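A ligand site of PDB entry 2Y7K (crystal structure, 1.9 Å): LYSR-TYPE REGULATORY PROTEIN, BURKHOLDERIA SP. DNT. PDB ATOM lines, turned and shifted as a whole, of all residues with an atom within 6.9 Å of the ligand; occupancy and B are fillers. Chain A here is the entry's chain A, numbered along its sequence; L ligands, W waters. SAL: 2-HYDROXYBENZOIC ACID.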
ATOM      1  N   MET A  14       1.948   4.470 -25.587  1.00  0.00           N
ATOM      2  CA  MET A  14       0.604   4.477 -26.178  1.00  0.00           C
ATOM      3  C   MET A  14       0.181   3.047 -26.448  1.00  0.00           C
ATOM      4  O   MET A  14       1.018   2.133 -26.382  1.00  0.00           O
ATOM      5  CB  MET A  14       0.559   5.262 -27.493  1.00  0.00           C
ATOM      6  CG  MET A  14       1.496   4.787 -28.554  1.00  0.00           C
ATOM      7  SD  MET A  14       1.450   5.766 -30.061  1.00  0.00           S
ATOM      8  CE  MET A  14       2.302   7.212 -29.437  1.00  0.00           C
ATOM      9  N   THR A  15      -1.097   2.870 -26.745  1.00  0.00           N
ATOM     10  CA  THR A  15      -1.660   1.524 -27.088  1.00  0.00           C
ATOM     11  C   THR A  15      -1.354   1.154 -28.536  1.00  0.00           C
ATOM     12  O   THR A  15      -0.861   1.989 -29.337  1.00  0.00           O
ATOM     13  CB  THR A  15      -3.226   1.525 -26.896  1.00  0.00           C
ATOM     14  OG1 THR A  15      -3.818   2.468 -27.780  1.00  0.00           O
ATOM     15  CG2 THR A  15      -3.586   1.935 -25.517  1.00  0.00           C
ATOM     16  N   ASP A  16      -1.638  -0.110 -28.897  1.00  0.00           N
ATOM     17  CA  ASP A  16      -1.691  -0.519 -30.299  1.00  0.00           C
ATOM     18  C   ASP A  16      -2.601   0.373 -31.163  1.00  0.00           C
ATOM     19  O   ASP A  16      -2.267   0.751 -32.295  1.00  0.00           O
ATOM     20  CB  ASP A  16      -2.048  -2.016 -30.393  1.00  0.00           C
ATOM     21  CG  ASP A  16      -3.303  -2.405 -29.568  1.00  0.00           C
ATOM     22  OD1 ASP A  16      -3.936  -1.567 -28.876  1.00  0.00           O
ATOM     23  OD2 ASP A  16      -3.669  -3.597 -29.607  1.00  0.00           O
ATOM     24  N   ILE A  17      -3.747   0.785 -30.625  1.00  0.00           N
ATOM     25  CA  ILE A  17      -4.595   1.709 -31.383  1.00  0.00           C
ATOM     26  C   ILE A  17      -3.862   3.027 -31.597  1.00  0.00           C
ATOM     27  O   ILE A  17      -3.861   3.556 -32.693  1.00  0.00           O
ATOM     28  CB  ILE A  17      -5.961   2.024 -30.664  1.00  0.00           C
ATOM     29  CG1 ILE A  17      -6.791   0.757 -30.516  1.00  0.00           C
ATOM     30  CG2 ILE A  17      -6.729   3.113 -31.432  1.00  0.00           C
ATOM     31  CD1 ILE A  17      -8.002   0.935 -29.540  1.00  0.00           C
ATOM     32  N   GLY A  18      -3.188   3.501 -30.556  1.00  0.00           N
ATOM     33  CA  GLY A  18      -2.430   4.771 -30.626  1.00  0.00           C
ATOM     34  C   GLY A  18      -1.375   4.707 -31.733  1.00  0.00           C
ATOM     35  O   GLY A  18      -1.252   5.616 -32.542  1.00  0.00           O
ATOM     36  N   GLU A  19      -0.631   3.601 -31.803  1.00  0.00           N
ATOM     37  CA  GLU A  19       0.358   3.453 -32.878  1.00  0.00           C
ATOM     38  C   GLU A  19      -0.207   3.549 -34.272  1.00  0.00           C
ATOM     39  O   GLU A  19       0.302   4.315 -35.112  1.00  0.00           O
ATOM     40  CB  GLU A  19       1.125   2.148 -32.735  1.00  0.00           C
ATOM     41  CG  GLU A  19       1.895   2.157 -31.453  1.00  0.00           C
ATOM     42  CD  GLU A  19       2.596   0.858 -31.165  1.00  0.00           C
ATOM     43  OE1 GLU A  19       2.509  -0.085 -32.011  1.00  0.00           O
ATOM     44  OE2 GLU A  19       3.222   0.787 -30.097  1.00  0.00           O
ATOM     45  N   TYR A  21      -2.951   4.944 -35.266  1.00  0.00           N
ATOM     46  CA  TYR A  21      -3.660   6.181 -35.438  1.00  0.00           C
ATOM     47  C   TYR A  21      -2.696   7.370 -35.451  1.00  0.00           C
ATOM     48  O   TYR A  21      -2.793   8.250 -36.307  1.00  0.00           O
ATOM     49  CB  TYR A  21      -4.673   6.340 -34.289  1.00  0.00           C
ATOM     50  CG  TYR A  21      -5.545   7.583 -34.376  1.00  0.00           C
ATOM     51  CD1 TYR A  21      -5.078   8.804 -33.952  1.00  0.00           C
ATOM     52  CD2 TYR A  21      -6.839   7.490 -34.877  1.00  0.00           C
ATOM     53  CE1 TYR A  21      -5.890   9.959 -34.036  1.00  0.00           C
ATOM     54  CE2 TYR A  21      -7.667   8.618 -34.954  1.00  0.00           C
ATOM     55  CZ  TYR A  21      -7.197   9.849 -34.531  1.00  0.00           C
ATOM     56  OH  TYR A  21      -8.033  10.980 -34.602  1.00  0.00           O
ATOM     57  N   PHE A  22      -1.808   7.434 -34.455  1.00  0.00           N
ATOM     58  CA  PHE A  22      -0.886   8.538 -34.357  1.00  0.00           C
ATOM     59  C   PHE A  22       0.362   8.436 -35.290  1.00  0.00           C
ATOM     60  O   PHE A  22       0.841   9.470 -35.798  1.00  0.00           O
ATOM     61  CB  PHE A  22      -0.387   8.690 -32.915  1.00  0.00           C
ATOM     62  CG  PHE A  22      -1.459   9.101 -31.942  1.00  0.00           C
ATOM     63  CD1 PHE A  22      -2.174  10.286 -32.139  1.00  0.00           C
ATOM     64  CD2 PHE A  22      -1.762   8.320 -30.841  1.00  0.00           C
ATOM     65  CE1 PHE A  22      -3.178  10.675 -31.243  1.00  0.00           C
ATOM     66  CE2 PHE A  22      -2.741   8.714 -29.925  1.00  0.00           C
ATOM     67  CZ  PHE A  22      -3.457   9.877 -30.134  1.00  0.00           C
ATOM     68  N   LEU A  62       0.135   8.910 -24.455  1.00  0.00           N
ATOM     69  CA  LEU A  62      -1.056   9.241 -25.190  1.00  0.00           C
ATOM     70  C   LEU A  62      -2.085   8.142 -24.992  1.00  0.00           C
ATOM     71  O   LEU A  62      -1.758   6.924 -25.093  1.00  0.00           O
ATOM     72  CB  LEU A  62      -0.765   9.359 -26.680  1.00  0.00           C
ATOM     73  CG  LEU A  62       0.146  10.565 -26.963  1.00  0.00           C
ATOM     74  CD1 LEU A  62       1.620  10.192 -27.027  1.00  0.00           C
ATOM     75  CD2 LEU A  62      -0.330  11.313 -28.154  1.00  0.00           C
ATOM     76  N   GLY A  63      -3.324   8.548 -24.760  1.00  0.00           N
ATOM     77  CA  GLY A  63      -4.443   7.595 -24.740  1.00  0.00           C
ATOM     78  C   GLY A  63      -5.471   7.970 -23.680  1.00  0.00           C
ATOM     79  O   GLY A  63      -5.587   9.136 -23.231  1.00  0.00           O
ATOM     80  N   LEU A  64      -6.198   6.932 -23.259  1.00  0.00           N
ATOM     81  CA  LEU A  64      -7.152   7.040 -22.185  1.00  0.00           C
ATOM     82  C   LEU A  64      -6.451   6.525 -20.978  1.00  0.00           C
ATOM     83  O   LEU A  64      -6.338   5.309 -20.778  1.00  0.00           O
ATOM     84  CB  LEU A  64      -8.397   6.169 -22.526  1.00  0.00           C
ATOM     85  CG  LEU A  64      -9.458   6.006 -21.435  1.00  0.00           C
ATOM     86  CD1 LEU A  64     -10.029   7.406 -21.092  1.00  0.00           C
ATOM     87  CD2 LEU A  64     -10.543   5.051 -21.949  1.00  0.00           C
ATOM     88  N   LEU A  65      -5.989   7.445 -20.122  1.00  0.00           N
ATOM     89  CA  LEU A  65      -5.078   7.063 -19.052  1.00  0.00           C
ATOM     90  C   LEU A  65      -5.469   7.775 -17.769  1.00  0.00           C
ATOM     91  O   LEU A  65      -4.825   8.762 -17.376  1.00  0.00           O
ATOM     92  CB  LEU A  65      -3.625   7.427 -19.483  1.00  0.00           C
ATOM     93  CG  LEU A  65      -3.140   6.731 -20.798  1.00  0.00           C
ATOM     94  CD1 LEU A  65      -1.810   7.349 -21.297  1.00  0.00           C
ATOM     95  CD2 LEU A  65      -2.952   5.279 -20.580  1.00  0.00           C
ATOM     96  N   PHE A  78      -8.925  14.590 -28.437  1.00  0.00           N
ATOM     97  CA  PHE A  78     -10.262  14.369 -29.005  1.00  0.00           C
ATOM     98  C   PHE A  78     -11.013  13.366 -28.148  1.00  0.00           C
ATOM     99  O   PHE A  78     -10.430  12.760 -27.205  1.00  0.00           O
ATOM    100  CB  PHE A  78     -10.197  13.884 -30.472  1.00  0.00           C
ATOM    101  CG  PHE A  78      -9.419  12.606 -30.659  1.00  0.00           C
ATOM    102  CD1 PHE A  78     -10.049  11.389 -30.544  1.00  0.00           C
ATOM    103  CD2 PHE A  78      -8.046  12.638 -30.944  1.00  0.00           C
ATOM    104  CE1 PHE A  78      -9.334  10.181 -30.710  1.00  0.00           C
ATOM    105  CE2 PHE A  78      -7.323  11.408 -31.105  1.00  0.00           C
ATOM    106  CZ  PHE A  78      -7.977  10.207 -30.998  1.00  0.00           C
ATOM    107  N   HIS A  80     -14.333  10.259 -28.260  1.00  0.00           N
ATOM    108  CA  HIS A  80     -15.111   9.361 -29.090  1.00  0.00           C
ATOM    109  C   HIS A  80     -15.800   8.346 -28.165  1.00  0.00           C
ATOM    110  O   HIS A  80     -15.727   8.470 -26.928  1.00  0.00           O
ATOM    111  CB  HIS A  80     -14.297   8.785 -30.262  1.00  0.00           C
ATOM    112  CG  HIS A  80     -13.105   7.979 -29.848  1.00  0.00           C
ATOM    113  ND1 HIS A  80     -12.811   6.769 -30.419  1.00  0.00           N
ATOM    114  CD2 HIS A  80     -12.204   8.164 -28.850  1.00  0.00           C
ATOM    115  CE1 HIS A  80     -11.714   6.265 -29.853  1.00  0.00           C
ATOM    116  NE2 HIS A  80     -11.337   7.100 -28.897  1.00  0.00           N
ATOM    117  N   THR A 115      -4.804   0.904 -18.980  1.00  0.00           N
ATOM    118  CA  THR A 115      -5.572   1.991 -19.609  1.00  0.00           C
ATOM    119  C   THR A 115      -6.967   2.120 -19.005  1.00  0.00           C
ATOM    120  O   THR A 115      -7.413   1.237 -18.282  1.00  0.00           O
ATOM    121  CB  THR A 115      -5.688   1.839 -21.137  1.00  0.00           C
ATOM    122  OG1 THR A 115      -6.639   0.822 -21.444  1.00  0.00           O
ATOM    123  CG2 THR A 115      -4.300   1.464 -21.734  1.00  0.00           C
ATOM    124  N   HIS A 117      -9.537   1.686 -20.564  1.00  0.00           N
ATOM    125  CA  HIS A 117     -10.409   0.727 -21.261  1.00  0.00           C
ATOM    126  C   HIS A 117     -10.608  -0.513 -20.436  1.00  0.00           C
ATOM    127  O   HIS A 117     -11.531  -1.308 -20.705  1.00  0.00           O
ATOM    128  CB  HIS A 117      -9.826   0.264 -22.567  1.00  0.00           C
ATOM    129  CG  HIS A 117      -9.568   1.365 -23.544  1.00  0.00           C
ATOM    130  ND1 HIS A 117     -10.575   2.117 -24.084  1.00  0.00           N
ATOM    131  CD2 HIS A 117      -8.412   1.809 -24.084  1.00  0.00           C
ATOM    132  CE1 HIS A 117     -10.051   2.981 -24.947  1.00  0.00           C
ATOM    133  NE2 HIS A 117      -8.746   2.789 -24.979  1.00  0.00           N
ATOM    134  N   PHE A 140      -6.479  -4.421 -28.087  1.00  0.00           N
ATOM    135  CA  PHE A 140      -7.462  -4.195 -29.140  1.00  0.00           C
ATOM    136  C   PHE A 140      -7.104  -4.659 -30.557  1.00  0.00           C
ATOM    137  O   PHE A 140      -7.926  -5.239 -31.275  1.00  0.00           O
ATOM    138  CB  PHE A 140      -7.866  -2.726 -29.147  1.00  0.00           C
ATOM    139  CG  PHE A 140      -8.836  -2.385 -28.054  1.00  0.00           C
ATOM    140  CD1 PHE A 140     -10.140  -2.860 -28.093  1.00  0.00           C
ATOM    141  CD2 PHE A 140      -8.416  -1.625 -26.955  1.00  0.00           C
ATOM    142  CE1 PHE A 140     -11.044  -2.602 -27.070  1.00  0.00           C
ATOM    143  CE2 PHE A 140      -9.297  -1.341 -25.908  1.00  0.00           C
ATOM    144  CZ  PHE A 140     -10.620  -1.811 -25.959  1.00  0.00           C
ATOM    145  N   PRO A 157     -13.239   1.043 -29.160  1.00  0.00           N
ATOM    146  CA  PRO A 157     -13.251   2.488 -29.424  1.00  0.00           C
ATOM    147  C   PRO A 157     -13.612   2.776 -30.874  1.00  0.00           C
ATOM    148  O   PRO A 157     -13.063   2.129 -31.814  1.00  0.00           O
ATOM    149  CB  PRO A 157     -11.790   2.895 -29.157  1.00  0.00           C
ATOM    150  CG  PRO A 157     -11.349   1.880 -28.073  1.00  0.00           C
ATOM    151  CD  PRO A 157     -11.935   0.621 -28.593  1.00  0.00           C
ATOM    152  N   GLN A 158     -14.548   3.697 -31.068  1.00  0.00           N
ATOM    153  CA  GLN A 158     -15.120   3.932 -32.422  1.00  0.00           C
ATOM    154  C   GLN A 158     -14.079   4.330 -33.480  1.00  0.00           C
ATOM    155  O   GLN A 158     -14.178   3.897 -34.648  1.00  0.00           O
ATOM    156  CB  GLN A 158     -16.205   5.031 -32.372  1.00  0.00           C
ATOM    157  CG  GLN A 158     -16.921   5.242 -33.713  1.00  0.00           C
ATOM    158  CD  GLN A 158     -16.332   6.361 -34.535  1.00  0.00           C
ATOM    159  OE1 GLN A 158     -15.694   7.287 -34.004  1.00  0.00           O
ATOM    160  NE2 GLN A 158     -16.546   6.310 -35.857  1.00  0.00           N
ATOM    161  N   ARG A 159     -13.142   5.209 -33.131  1.00  0.00           N
ATOM    162  CA  ARG A 159     -12.133   5.629 -34.134  1.00  0.00           C
ATOM    163  C   ARG A 159     -11.258   4.464 -34.590  1.00  0.00           C
ATOM    164  O   ARG A 159     -10.748   4.466 -35.729  1.00  0.00           O
ATOM    165  CB  ARG A 159     -11.269   6.785 -33.624  1.00  0.00           C
ATOM    166  CG  ARG A 159     -12.114   8.050 -33.422  1.00  0.00           C
ATOM    167  CD  ARG A 159     -11.305   9.297 -33.478  1.00  0.00           C
ATOM    168  NE  ARG A 159     -12.197  10.447 -33.316  1.00  0.00           N
ATOM    169  CZ  ARG A 159     -11.856  11.710 -33.548  1.00  0.00           C
ATOM    170  NH1 ARG A 159     -10.636  12.010 -33.975  1.00  0.00           N
ATOM    171  NH2 ARG A 159     -12.742  12.675 -33.348  1.00  0.00           N
ATOM    172  N   PHE A 160     -11.064   3.500 -33.693  1.00  0.00           N
ATOM    173  CA  PHE A 160     -10.433   2.239 -34.047  1.00  0.00           C
ATOM    174  C   PHE A 160     -11.369   1.408 -34.929  1.00  0.00           C
ATOM    175  O   PHE A 160     -10.978   0.918 -35.984  1.00  0.00           O
ATOM    176  CB  PHE A 160     -10.004   1.466 -32.784  1.00  0.00           C
ATOM    177  CG  PHE A 160      -9.659   0.037 -33.030  1.00  0.00           C
ATOM    178  CD1 PHE A 160      -8.535  -0.301 -33.795  1.00  0.00           C
ATOM    179  CD2 PHE A 160     -10.459  -0.977 -32.541  1.00  0.00           C
ATOM    180  CE1 PHE A 160      -8.205  -1.664 -34.038  1.00  0.00           C
ATOM    181  CE2 PHE A 160     -10.162  -2.310 -32.774  1.00  0.00           C
ATOM    182  CZ  PHE A 160      -9.043  -2.677 -33.514  1.00  0.00           C
ATOM    183  N   ILE A 182     -14.799   8.375 -24.397  1.00  0.00           N
ATOM    184  CA  ILE A 182     -13.367   8.050 -24.375  1.00  0.00           C
ATOM    185  C   ILE A 182     -12.643   9.356 -24.655  1.00  0.00           C
ATOM    186  O   ILE A 182     -12.713   9.861 -25.758  1.00  0.00           O
ATOM    187  CB  ILE A 182     -13.008   7.027 -25.480  1.00  0.00           C
ATOM    188  CG1 ILE A 182     -13.727   5.697 -25.240  1.00  0.00           C
ATOM    189  CG2 ILE A 182     -11.448   6.776 -25.562  1.00  0.00           C
ATOM    190  CD1 ILE A 182     -13.929   4.880 -26.508  1.00  0.00           C
ATOM    191  N   ILE A 184      -9.272  11.010 -25.351  1.00  0.00           N
ATOM    192  CA  ILE A 184      -7.867  10.728 -25.728  1.00  0.00           C
ATOM    193  C   ILE A 184      -7.039  11.989 -25.503  1.00  0.00           C
ATOM    194  O   ILE A 184      -7.227  13.006 -26.200  1.00  0.00           O
ATOM    195  CB  ILE A 184      -7.731  10.270 -27.153  1.00  0.00           C
ATOM    196  CG1 ILE A 184      -8.508   8.964 -27.390  1.00  0.00           C
ATOM    197  CG2 ILE A 184      -6.207  10.048 -27.561  1.00  0.00           C
ATOM    198  CD1 ILE A 184      -8.202   7.764 -26.336  1.00  0.00           C
HETATM  199  C1' SAL L   1      -6.623   4.770 -27.483  1.00  0.00           C
HETATM  200  O1' SAL L   1      -7.638   4.149 -27.041  1.00  0.00           O
HETATM  201  O2' SAL L   1      -5.528   4.774 -26.907  1.00  0.00           O
HETATM  202  C1  SAL L   1      -6.749   5.565 -28.795  1.00  0.00           C
HETATM  203  C2  SAL L   1      -7.976   5.643 -29.426  1.00  0.00           C
HETATM  204  C3  SAL L   1      -8.105   6.342 -30.640  1.00  0.00           C
HETATM  205  C4  SAL L   1      -6.981   6.957 -31.217  1.00  0.00           C
HETATM  206  C5  SAL L   1      -5.741   6.876 -30.582  1.00  0.00           C
HETATM  207  C6  SAL L   1      -5.622   6.190 -29.372  1.00  0.00           C
HETATM  208  O2  SAL L   1      -9.050   5.028 -28.809  1.00  0.00           O
HETATM  209  O   HOH W   1      -2.774   5.340 -27.216  1.00  0.00           O
HETATM  210  O   HOH W   2      -5.531   4.334 -24.147  1.00  0.00           O
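The backbone NH (N) of Ile 184 sits at hydrogen-bond distance from the backbone carbonyl oxygen (O) of Phe 78 (2.8 Å). OG1 of Thr 15 lies within hydrogen-bond range of N of Gly 18, 3.0 Å away. OH of Tyr 21 lies within hydrogen-bond range of NH1 of Arg 159 (2.9 Å). A ring nitrogen (ND1) of His 80 lies within hydrogen-bond range of the backbone NH of Arg 159 (3.1 Å). OG1 of Thr 115 lies close to N of His 117. The side-chain hydroxyl (OG1) of Thr 15 sits close to the backbone NH (N) of Ile 17. N of Ile 182 sits at hydrogen-bond distance from O of His 80.
Water W2 bridges O2' of the ligand and N of Leu 64. Water W1 lies within hydrogen-bond range of an oxygen (O2') of the ligand, the backbone carbonyl oxygen of Leu 62 and the backbone NH of Thr 15.
The side-chain hydroxyl of Thr 15 sits at hydrogen-bond distance from an oxygen (O2') of the ligand, at 3.0 Å. A ring nitrogen (NE2) of His 117 is in hydrogen-bond range of an oxygen (O1') of the ligand, at 2.7 Å. A ring nitrogen (NE2) of His 80 sits at hydrogen-bond distance from an oxygen (O2) of the ligand (3.1 Å).
Ile 17 touches the ligand. Gly 18 touches the ligand. Tyr 21 touches the ligand. Phe 22 touches the ligand. Gly 63 touches the ligand. Phe 78 touches the ligand. CB of Pro 157 touches O2 of the ligand, 3.5 Å away. CD1 of Ile 184 touches C1' of the ligand, at 3.6 Å. Hydrophobic or aromatic side chains that line the ligand: Ile 17, Tyr 21, Phe 22, Phe 78, His 80, His 117, Pro 157 and Ile 184. Within 4 Å of the ligand: Thr 15, Ile 17, Gly 18, Tyr 21, Phe 22, Gly 63, Phe 78, His 80, His 117, Pro 157 and Ile 184. The nearest printed residue that does not touch the ligand is Leu 64 (4.3 Å).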
